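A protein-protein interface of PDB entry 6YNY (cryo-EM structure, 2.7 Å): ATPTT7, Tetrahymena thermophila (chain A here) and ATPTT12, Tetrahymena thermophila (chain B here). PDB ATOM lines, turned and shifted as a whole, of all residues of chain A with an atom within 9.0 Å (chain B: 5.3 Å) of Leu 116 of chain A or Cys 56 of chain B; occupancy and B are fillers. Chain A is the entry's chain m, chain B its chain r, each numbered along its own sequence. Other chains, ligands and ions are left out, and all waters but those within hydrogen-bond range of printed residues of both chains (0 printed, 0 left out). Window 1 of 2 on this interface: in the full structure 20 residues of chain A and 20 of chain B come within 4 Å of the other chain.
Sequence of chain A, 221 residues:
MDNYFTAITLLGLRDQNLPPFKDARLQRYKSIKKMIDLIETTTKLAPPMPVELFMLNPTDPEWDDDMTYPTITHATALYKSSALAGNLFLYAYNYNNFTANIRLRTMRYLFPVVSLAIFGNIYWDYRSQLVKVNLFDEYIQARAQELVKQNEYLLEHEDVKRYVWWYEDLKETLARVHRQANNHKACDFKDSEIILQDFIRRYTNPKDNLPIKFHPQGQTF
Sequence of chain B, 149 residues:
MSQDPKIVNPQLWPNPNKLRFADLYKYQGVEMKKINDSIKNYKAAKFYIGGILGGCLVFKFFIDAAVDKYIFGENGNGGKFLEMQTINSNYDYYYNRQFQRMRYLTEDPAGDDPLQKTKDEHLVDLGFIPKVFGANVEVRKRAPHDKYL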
ATOM      1  N   LEU A  84      21.158  -1.551  14.022  1.00  0.00           N
ATOM      2  CA  LEU A  84      20.293  -1.127  12.929  1.00  0.00           C
ATOM      3  C   LEU A  84      19.252  -2.191  12.614  1.00  0.00           C
ATOM      4  O   LEU A  84      18.073  -1.878  12.414  1.00  0.00           O
ATOM      5  CB  LEU A  84      21.135  -0.816  11.696  1.00  0.00           C
ATOM      6  CG  LEU A  84      20.379  -0.443  10.425  1.00  0.00           C
ATOM      7  CD1 LEU A  84      19.551   0.800  10.635  1.00  0.00           C
ATOM      8  CD2 LEU A  84      21.354  -0.248   9.292  1.00  0.00           C
ATOM      9  N   LEU A  88      14.925  -2.316  12.624  1.00  0.00           N
ATOM     10  CA  LEU A  88      14.052  -2.911  11.620  1.00  0.00           C
ATOM     11  C   LEU A  88      13.077  -3.896  12.249  1.00  0.00           C
ATOM     12  O   LEU A  88      11.928  -4.004  11.810  1.00  0.00           O
ATOM     13  CB  LEU A  88      14.889  -3.595  10.546  1.00  0.00           C
ATOM     14  CG  LEU A  88      15.901  -2.691   9.849  1.00  0.00           C
ATOM     15  CD1 LEU A  88      16.733  -3.472   8.863  1.00  0.00           C
ATOM     16  CD2 LEU A  88      15.209  -1.550   9.155  1.00  0.00           C
ATOM     17  N   LEU A 110      10.256   9.085   7.779  1.00  0.00           N
ATOM     18  CA  LEU A 110      11.658   9.410   7.978  1.00  0.00           C
ATOM     19  C   LEU A 110      12.470   8.284   8.598  1.00  0.00           C
ATOM     20  O   LEU A 110      13.695   8.410   8.688  1.00  0.00           O
ATOM     21  CB  LEU A 110      11.784  10.665   8.850  1.00  0.00           C
ATOM     22  CG  LEU A 110      10.907  11.838   8.413  1.00  0.00           C
ATOM     23  CD1 LEU A 110      11.164  13.042   9.277  1.00  0.00           C
ATOM     24  CD2 LEU A 110      11.129  12.178   6.959  1.00  0.00           C
ATOM     25  N   PHE A 111      11.833   7.201   9.032  1.00  0.00           N
ATOM     26  CA  PHE A 111      12.590   6.039   9.484  1.00  0.00           C
ATOM     27  C   PHE A 111      13.569   5.542   8.430  1.00  0.00           C
ATOM     28  O   PHE A 111      14.723   5.249   8.789  1.00  0.00           O
ATOM     29  CB  PHE A 111      11.624   4.924   9.900  1.00  0.00           C
ATOM     30  CG  PHE A 111      12.301   3.674  10.371  1.00  0.00           C
ATOM     31  CD1 PHE A 111      12.592   3.494  11.706  1.00  0.00           C
ATOM     32  CD2 PHE A 111      12.635   2.673   9.482  1.00  0.00           C
ATOM     33  CE1 PHE A 111      13.208   2.348  12.141  1.00  0.00           C
ATOM     34  CE2 PHE A 111      13.251   1.528   9.913  1.00  0.00           C
ATOM     35  CZ  PHE A 111      13.538   1.365  11.244  1.00  0.00           C
ATOM     36  N   PRO A 112      13.202   5.418   7.151  1.00  0.00           N
ATOM     37  CA  PRO A 112      14.179   4.930   6.171  1.00  0.00           C
ATOM     38  C   PRO A 112      15.280   5.927   5.874  1.00  0.00           C
ATOM     39  O   PRO A 112      16.409   5.516   5.584  1.00  0.00           O
ATOM     40  CB  PRO A 112      13.320   4.648   4.933  1.00  0.00           C
ATOM     41  CG  PRO A 112      12.149   5.509   5.080  1.00  0.00           C
ATOM     42  CD  PRO A 112      11.889   5.665   6.534  1.00  0.00           C
ATOM     43  N   VAL A 113      14.989   7.225   5.940  1.00  0.00           N
ATOM     44  CA  VAL A 113      16.032   8.226   5.742  1.00  0.00           C
ATOM     45  C   VAL A 113      17.073   8.127   6.847  1.00  0.00           C
ATOM     46  O   VAL A 113      18.280   8.202   6.593  1.00  0.00           O
ATOM     47  CB  VAL A 113      15.408   9.629   5.672  1.00  0.00           C
ATOM     48  CG1 VAL A 113      16.481  10.679   5.550  1.00  0.00           C
ATOM     49  CG2 VAL A 113      14.451   9.714   4.509  1.00  0.00           C
ATOM     50  N   VAL A 114      16.624   7.959   8.089  1.00  0.00           N
ATOM     51  CA  VAL A 114      17.555   7.772   9.194  1.00  0.00           C
ATOM     52  C   VAL A 114      18.270   6.435   9.066  1.00  0.00           C
ATOM     53  O   VAL A 114      19.454   6.314   9.401  1.00  0.00           O
ATOM     54  CB  VAL A 114      16.811   7.894  10.535  1.00  0.00           C
ATOM     55  CG1 VAL A 114      17.723   7.555  11.690  1.00  0.00           C
ATOM     56  CG2 VAL A 114      16.260   9.285  10.702  1.00  0.00           C
ATOM     57  N   SER A 115      17.568   5.411   8.581  1.00  0.00           N
ATOM     58  CA  SER A 115      18.186   4.101   8.424  1.00  0.00           C
ATOM     59  C   SER A 115      19.292   4.128   7.379  1.00  0.00           C
ATOM     60  O   SER A 115      20.342   3.503   7.563  1.00  0.00           O
ATOM     61  CB  SER A 115      17.127   3.064   8.057  1.00  0.00           C
ATOM     62  OG  SER A 115      16.108   3.008   9.032  1.00  0.00           O
ATOM     63  N   LEU A 116      19.078   4.844   6.273  1.00  0.00           N
ATOM     64  CA  LEU A 116      20.118   4.949   5.256  1.00  0.00           C
ATOM     65  C   LEU A 116      21.302   5.758   5.761  1.00  0.00           C
ATOM     66  O   LEU A 116      22.459   5.393   5.519  1.00  0.00           O
ATOM     67  CB  LEU A 116      19.556   5.581   3.983  1.00  0.00           C
ATOM     68  CG  LEU A 116      18.511   4.789   3.201  1.00  0.00           C
ATOM     69  CD1 LEU A 116      18.178   5.504   1.914  1.00  0.00           C
ATOM     70  CD2 LEU A 116      18.995   3.400   2.913  1.00  0.00           C
ATOM     71  N   ALA A 117      21.037   6.858   6.462  1.00  0.00           N
ATOM     72  CA  ALA A 117      22.121   7.646   7.030  1.00  0.00           C
ATOM     73  C   ALA A 117      22.923   6.840   8.038  1.00  0.00           C
ATOM     74  O   ALA A 117      24.129   7.057   8.188  1.00  0.00           O
ATOM     75  CB  ALA A 117      21.562   8.907   7.680  1.00  0.00           C
ATOM     76  N   ILE A 118      22.274   5.912   8.739  1.00  0.00           N
ATOM     77  CA  ILE A 118      22.988   5.048   9.670  1.00  0.00           C
ATOM     78  C   ILE A 118      23.794   4.004   8.910  1.00  0.00           C
ATOM     79  O   ILE A 118      24.964   3.754   9.219  1.00  0.00           O
ATOM     80  CB  ILE A 118      21.998   4.401  10.654  1.00  0.00           C
ATOM     81  CG1 ILE A 118      21.437   5.461  11.601  1.00  0.00           C
ATOM     82  CG2 ILE A 118      22.670   3.293  11.438  1.00  0.00           C
ATOM     83  CD1 ILE A 118      20.220   5.026  12.360  1.00  0.00           C
ATOM     84  N   PHE A 119      23.181   3.377   7.903  1.00  0.00           N
ATOM     85  CA  PHE A 119      23.919   2.440   7.063  1.00  0.00           C
ATOM     86  C   PHE A 119      25.107   3.116   6.401  1.00  0.00           C
ATOM     87  O   PHE A 119      26.194   2.536   6.316  1.00  0.00           O
ATOM     88  CB  PHE A 119      23.000   1.840   6.004  1.00  0.00           C
ATOM     89  CG  PHE A 119      23.730   1.120   4.913  1.00  0.00           C
ATOM     90  CD1 PHE A 119      24.097  -0.200   5.069  1.00  0.00           C
ATOM     91  CD2 PHE A 119      24.056   1.762   3.735  1.00  0.00           C
ATOM     92  CE1 PHE A 119      24.771  -0.861   4.072  1.00  0.00           C
ATOM     93  CE2 PHE A 119      24.731   1.103   2.740  1.00  0.00           C
ATOM     94  CZ  PHE A 119      25.087  -0.209   2.909  1.00  0.00           C
ATOM     95  N   GLY A 120      24.918   4.345   5.923  1.00  0.00           N
ATOM     96  CA  GLY A 120      26.003   5.039   5.256  1.00  0.00           C
ATOM     97  C   GLY A 120      27.202   5.248   6.155  1.00  0.00           C
ATOM     98  O   GLY A 120      28.346   5.076   5.731  1.00  0.00           O
ATOM     99  N   ASN A 121      26.959   5.621   7.409  1.00  0.00           N
ATOM    100  CA  ASN A 121      28.057   5.796   8.347  1.00  0.00           C
ATOM    101  C   ASN A 121      28.761   4.475   8.619  1.00  0.00           C
ATOM    102  O   ASN A 121      29.993   4.426   8.701  1.00  0.00           O
ATOM    103  CB  ASN A 121      27.537   6.408   9.646  1.00  0.00           C
ATOM    104  CG  ASN A 121      28.524   6.284  10.781  1.00  0.00           C
ATOM    105  OD1 ASN A 121      28.298   5.546  11.738  1.00  0.00           O
ATOM    106  ND2 ASN A 121      29.634   6.991  10.673  1.00  0.00           N
ATOM    107  N   ILE A 122      27.995   3.394   8.755  1.00  0.00           N
ATOM    108  CA  ILE A 122      28.586   2.090   9.031  1.00  0.00           C
ATOM    109  C   ILE A 122      29.465   1.651   7.869  1.00  0.00           C
ATOM    110  O   ILE A 122      30.613   1.232   8.059  1.00  0.00           O
ATOM    111  CB  ILE A 122      27.487   1.056   9.328  1.00  0.00           C
ATOM    112  CG1 ILE A 122      26.717   1.450  10.585  1.00  0.00           C
ATOM    113  CG2 ILE A 122      28.086  -0.324   9.487  1.00  0.00           C
ATOM    114  CD1 ILE A 122      25.477   0.640  10.815  1.00  0.00           C
ATOM    115  N   TYR A 123      28.941   1.737   6.647  1.00  0.00           N
ATOM    116  CA  TYR A 123      29.697   1.280   5.489  1.00  0.00           C
ATOM    117  C   TYR A 123      30.804   2.256   5.115  1.00  0.00           C
ATOM    118  O   TYR A 123      31.884   1.834   4.687  1.00  0.00           O
ATOM    119  CB  TYR A 123      28.761   1.062   4.305  1.00  0.00           C
ATOM    120  CG  TYR A 123      29.455   0.463   3.113  1.00  0.00           C
ATOM    121  CD1 TYR A 123      29.846  -0.864   3.116  1.00  0.00           C
ATOM    122  CD2 TYR A 123      29.723   1.220   1.989  1.00  0.00           C
ATOM    123  CE1 TYR A 123      30.487  -1.415   2.036  1.00  0.00           C
ATOM    124  CE2 TYR A 123      30.361   0.678   0.908  1.00  0.00           C
ATOM    125  CZ  TYR A 123      30.740  -0.641   0.934  1.00  0.00           C
ATOM    126  OH  TYR A 123      31.379  -1.185  -0.152  1.00  0.00           O
ATOM    127  N   TRP A 124      30.560   3.556   5.262  1.00  0.00           N
ATOM    128  CA  TRP A 124      31.601   4.538   4.987  1.00  0.00           C
ATOM    129  C   TRP A 124      32.850   4.249   5.804  1.00  0.00           C
ATOM    130  O   TRP A 124      33.964   4.216   5.271  1.00  0.00           O
ATOM    131  CB  TRP A 124      31.081   5.944   5.278  1.00  0.00           C
ATOM    132  CG  TRP A 124      32.101   7.010   5.085  1.00  0.00           C
ATOM    133  CD1 TRP A 124      33.087   7.361   5.950  1.00  0.00           C
ATOM    134  CD2 TRP A 124      32.234   7.872   3.955  1.00  0.00           C
ATOM    135  NE1 TRP A 124      33.834   8.382   5.428  1.00  0.00           N
ATOM    136  CE2 TRP A 124      33.327   8.716   4.202  1.00  0.00           C
ATOM    137  CE3 TRP A 124      31.537   8.010   2.756  1.00  0.00           C
ATOM    138  CZ2 TRP A 124      33.737   9.682   3.299  1.00  0.00           C
ATOM    139  CZ3 TRP A 124      31.947   8.968   1.862  1.00  0.00           C
ATOM    140  CH2 TRP A 124      33.035   9.793   2.137  1.00  0.00           C
ATOM    141  N   GLY B  51      12.662  -2.541   0.830  1.00  0.00           N
ATOM    142  CA  GLY B  51      12.946  -1.292   0.151  1.00  0.00           C
ATOM    143  C   GLY B  51      14.085  -0.527   0.788  1.00  0.00           C
ATOM    144  O   GLY B  51      14.852   0.146   0.097  1.00  0.00           O
ATOM    145  N   ILE B  52      14.208  -0.613   2.112  1.00  0.00           N
ATOM    146  CA  ILE B  52      15.319   0.027   2.803  1.00  0.00           C
ATOM    147  C   ILE B  52      16.626  -0.674   2.465  1.00  0.00           C
ATOM    148  O   ILE B  52      17.619  -0.033   2.103  1.00  0.00           O
ATOM    149  CB  ILE B  52      15.057   0.043   4.318  1.00  0.00           C
ATOM    150  CG1 ILE B  52      13.887   0.968   4.629  1.00  0.00           C
ATOM    151  CG2 ILE B  52      16.301   0.466   5.073  1.00  0.00           C
ATOM    152  CD1 ILE B  52      13.424   0.919   6.053  1.00  0.00           C
ATOM    153  N   LEU B  53      16.646  -2.002   2.579  1.00  0.00           N
ATOM    154  CA  LEU B  53      17.853  -2.747   2.248  1.00  0.00           C
ATOM    155  C   LEU B  53      18.230  -2.557   0.787  1.00  0.00           C
ATOM    156  O   LEU B  53      19.416  -2.461   0.451  1.00  0.00           O
ATOM    157  CB  LEU B  53      17.651  -4.226   2.562  1.00  0.00           C
ATOM    158  CG  LEU B  53      17.313  -4.544   4.018  1.00  0.00           C
ATOM    159  CD1 LEU B  53      17.093  -6.024   4.186  1.00  0.00           C
ATOM    160  CD2 LEU B  53      18.402  -4.064   4.952  1.00  0.00           C
ATOM    161  N   GLY B  54      17.237  -2.500  -0.097  1.00  0.00           N
ATOM    162  CA  GLY B  54      17.524  -2.198  -1.486  1.00  0.00           C
ATOM    163  C   GLY B  54      18.137  -0.823  -1.656  1.00  0.00           C
ATOM    164  O   GLY B  54      19.010  -0.621  -2.502  1.00  0.00           O
ATOM    165  N   GLY B  55      17.687   0.142  -0.855  1.00  0.00           N
ATOM    166  CA  GLY B  55      18.303   1.454  -0.882  1.00  0.00           C
ATOM    167  C   GLY B  55      19.712   1.441  -0.324  1.00  0.00           C
ATOM    168  O   GLY B  55      20.588   2.161  -0.810  1.00  0.00           O
ATOM    169  N   CYS B  56      19.951   0.622   0.701  1.00  0.00           N
ATOM    170  CA  CYS B  56      21.301   0.490   1.238  1.00  0.00           C
ATOM    171  C   CYS B  56      22.238  -0.129   0.213  1.00  0.00           C
ATOM    172  O   CYS B  56      23.411   0.249   0.126  1.00  0.00           O
ATOM    173  CB  CYS B  56      21.281  -0.348   2.514  1.00  0.00           C
ATOM    174  SG  CYS B  56      20.531   0.451   3.945  1.00  0.00           S
ATOM    175  N   LEU B  57      21.739  -1.081  -0.574  1.00  0.00           N
ATOM    176  CA  LEU B  57      22.571  -1.709  -1.592  1.00  0.00           C
ATOM    177  C   LEU B  57      22.906  -0.730  -2.709  1.00  0.00           C
ATOM    178  O   LEU B  57      24.015  -0.754  -3.252  1.00  0.00           O
ATOM    179  CB  LEU B  57      21.868  -2.943  -2.152  1.00  0.00           C
ATOM    180  CG  LEU B  57      22.609  -3.719  -3.236  1.00  0.00           C
ATOM    181  CD1 LEU B  57      23.922  -4.255  -2.711  1.00  0.00           C
ATOM    182  CD2 LEU B  57      21.745  -4.847  -3.742  1.00  0.00           C
ATOM    183  N   VAL B  58      21.958   0.135  -3.065  1.00  0.00           N
ATOM    184  CA  VAL B  58      22.221   1.147  -4.080  1.00  0.00           C
ATOM    185  C   VAL B  58      23.096   2.254  -3.513  1.00  0.00           C
ATOM    186  O   VAL B  58      24.022   2.735  -4.175  1.00  0.00           O
ATOM    187  CB  VAL B  58      20.895   1.699  -4.627  1.00  0.00           C
ATOM    188  CG1 VAL B  58      21.149   2.847  -5.570  1.00  0.00           C
ATOM    189  CG2 VAL B  58      20.116   0.604  -5.320  1.00  0.00           C
ATOM    190  N   PHE B  59      22.817   2.677  -2.281  1.00  0.00           N
ATOM    191  CA  PHE B  59      23.626   3.702  -1.641  1.00  0.00           C
ATOM    192  C   PHE B  59      25.058   3.234  -1.429  1.00  0.00           C
ATOM    193  O   PHE B  59      25.959   4.064  -1.276  1.00  0.00           O
ATOM    194  CB  PHE B  59      22.986   4.083  -0.304  1.00  0.00           C
ATOM    195  CG  PHE B  59      23.477   5.377   0.279  1.00  0.00           C
ATOM    196  CD1 PHE B  59      24.155   6.304  -0.487  1.00  0.00           C
ATOM    197  CD2 PHE B  59      23.251   5.661   1.610  1.00  0.00           C
ATOM    198  CE1 PHE B  59      24.591   7.485   0.064  1.00  0.00           C
ATOM    199  CE2 PHE B  59      23.686   6.837   2.163  1.00  0.00           C
ATOM    200  CZ  PHE B  59      24.357   7.751   1.391  1.00  0.00           C
ATOM    201  N   LYS B  60      25.280   1.921  -1.423  1.00  0.00           N
ATOM    202  CA  LYS B  60      26.615   1.381  -1.201  1.00  0.00           C
ATOM    203  C   LYS B  60      27.564   1.753  -2.333  1.00  0.00           C
ATOM    204  O   LYS B  60      28.755   1.983  -2.100  1.00  0.00           O
ATOM    205  CB  LYS B  60      26.529  -0.135  -1.037  1.00  0.00           C
ATOM    206  CG  LYS B  60      27.851  -0.867  -1.087  1.00  0.00           C
ATOM    207  CD  LYS B  60      28.111  -1.445  -2.463  1.00  0.00           C
ATOM    208  CE  LYS B  60      29.420  -2.202  -2.514  1.00  0.00           C
ATOM    209  NZ  LYS B  60      29.417  -3.365  -1.604  1.00  0.00           N
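Of chain B, only Ile 52 (3.8 Å), Gly 55 (3.9 Å), Cys 56 (3.5 Å) and Phe 59 (3.9 Å) come within 4 Å of Leu 116 of chain A.
Cys 56 of chain B touches just these residues of chain A: Leu 116 and Phe 119.
No residue of chain A comes within 4 Å of Gly 54 of chain B.
Gly 55 of chain B touches one residue of chain A.
Of the printed residues of chain B, Phe 111 of chain A touches Ile 52.
Of the printed residues of chain A, Lys 60 of chain B touches Tyr 123.
Printed residues of chain A within 4 Å of Phe 59 of chain B: Leu 116.
Of the printed residues of chain B, Phe 119 of chain A touches Cys 56.
Printed residues of chain B within 4 Å of Pro 112 of chain A: Ile 52.
The side-chain sulfur of Cys 56 of chain B lies within hydrogen-bond range of the backbone carbonyl oxygen of Ile 52 of chain B.
The side-chain hydroxyl (OG) of Ser 115 of chain A lies within hydrogen-bond range of the backbone carbonyl oxygen (O) of Phe 111 of chain A, 2.6 Å away.
Of the 10 printed residues of chain B, 5 touch a printed residue of chain A.
Printed residues of chain B that touch a printed residue of chain A: Ile 52, Gly 55, Cys 56, Phe 59 and Lys 60.
Hydrophobic or aromatic side chains of chain B that line the printed part of chain A: Ile 52 and Phe 59.
Of the 17 printed residues of chain A, 5 touch a printed residue of chain B.
Hydrophobic or aromatic side chains of chain A within 4 Å of the printed part of chain B: Phe 111, Pro 112, Leu 116, Phe 119 and Tyr 123.
Among the printed residues, 8 pairs touch across the chains.
The side-chain hydroxyl (OH) of Tyr 123 of chain A lies close to the side-chain amino group (NZ) of Lys 60 of chain B, 3.3 Å away.
Among the printed residues, pairs that only touch across the chains: Phe 111 of chain A with Ile 52 of chain B, Pro 112 of chain A with Ile 52 of chain B, Leu 116 of chain A with Ile 52 of chain B, Leu 116 of chain A with Gly 55 of chain B, Leu 116 of chain A with Cys 56 of chain B, Leu 116 of chain A with Phe 59 of chain B and Phe 119 of chain A with Cys 56 of chain B.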
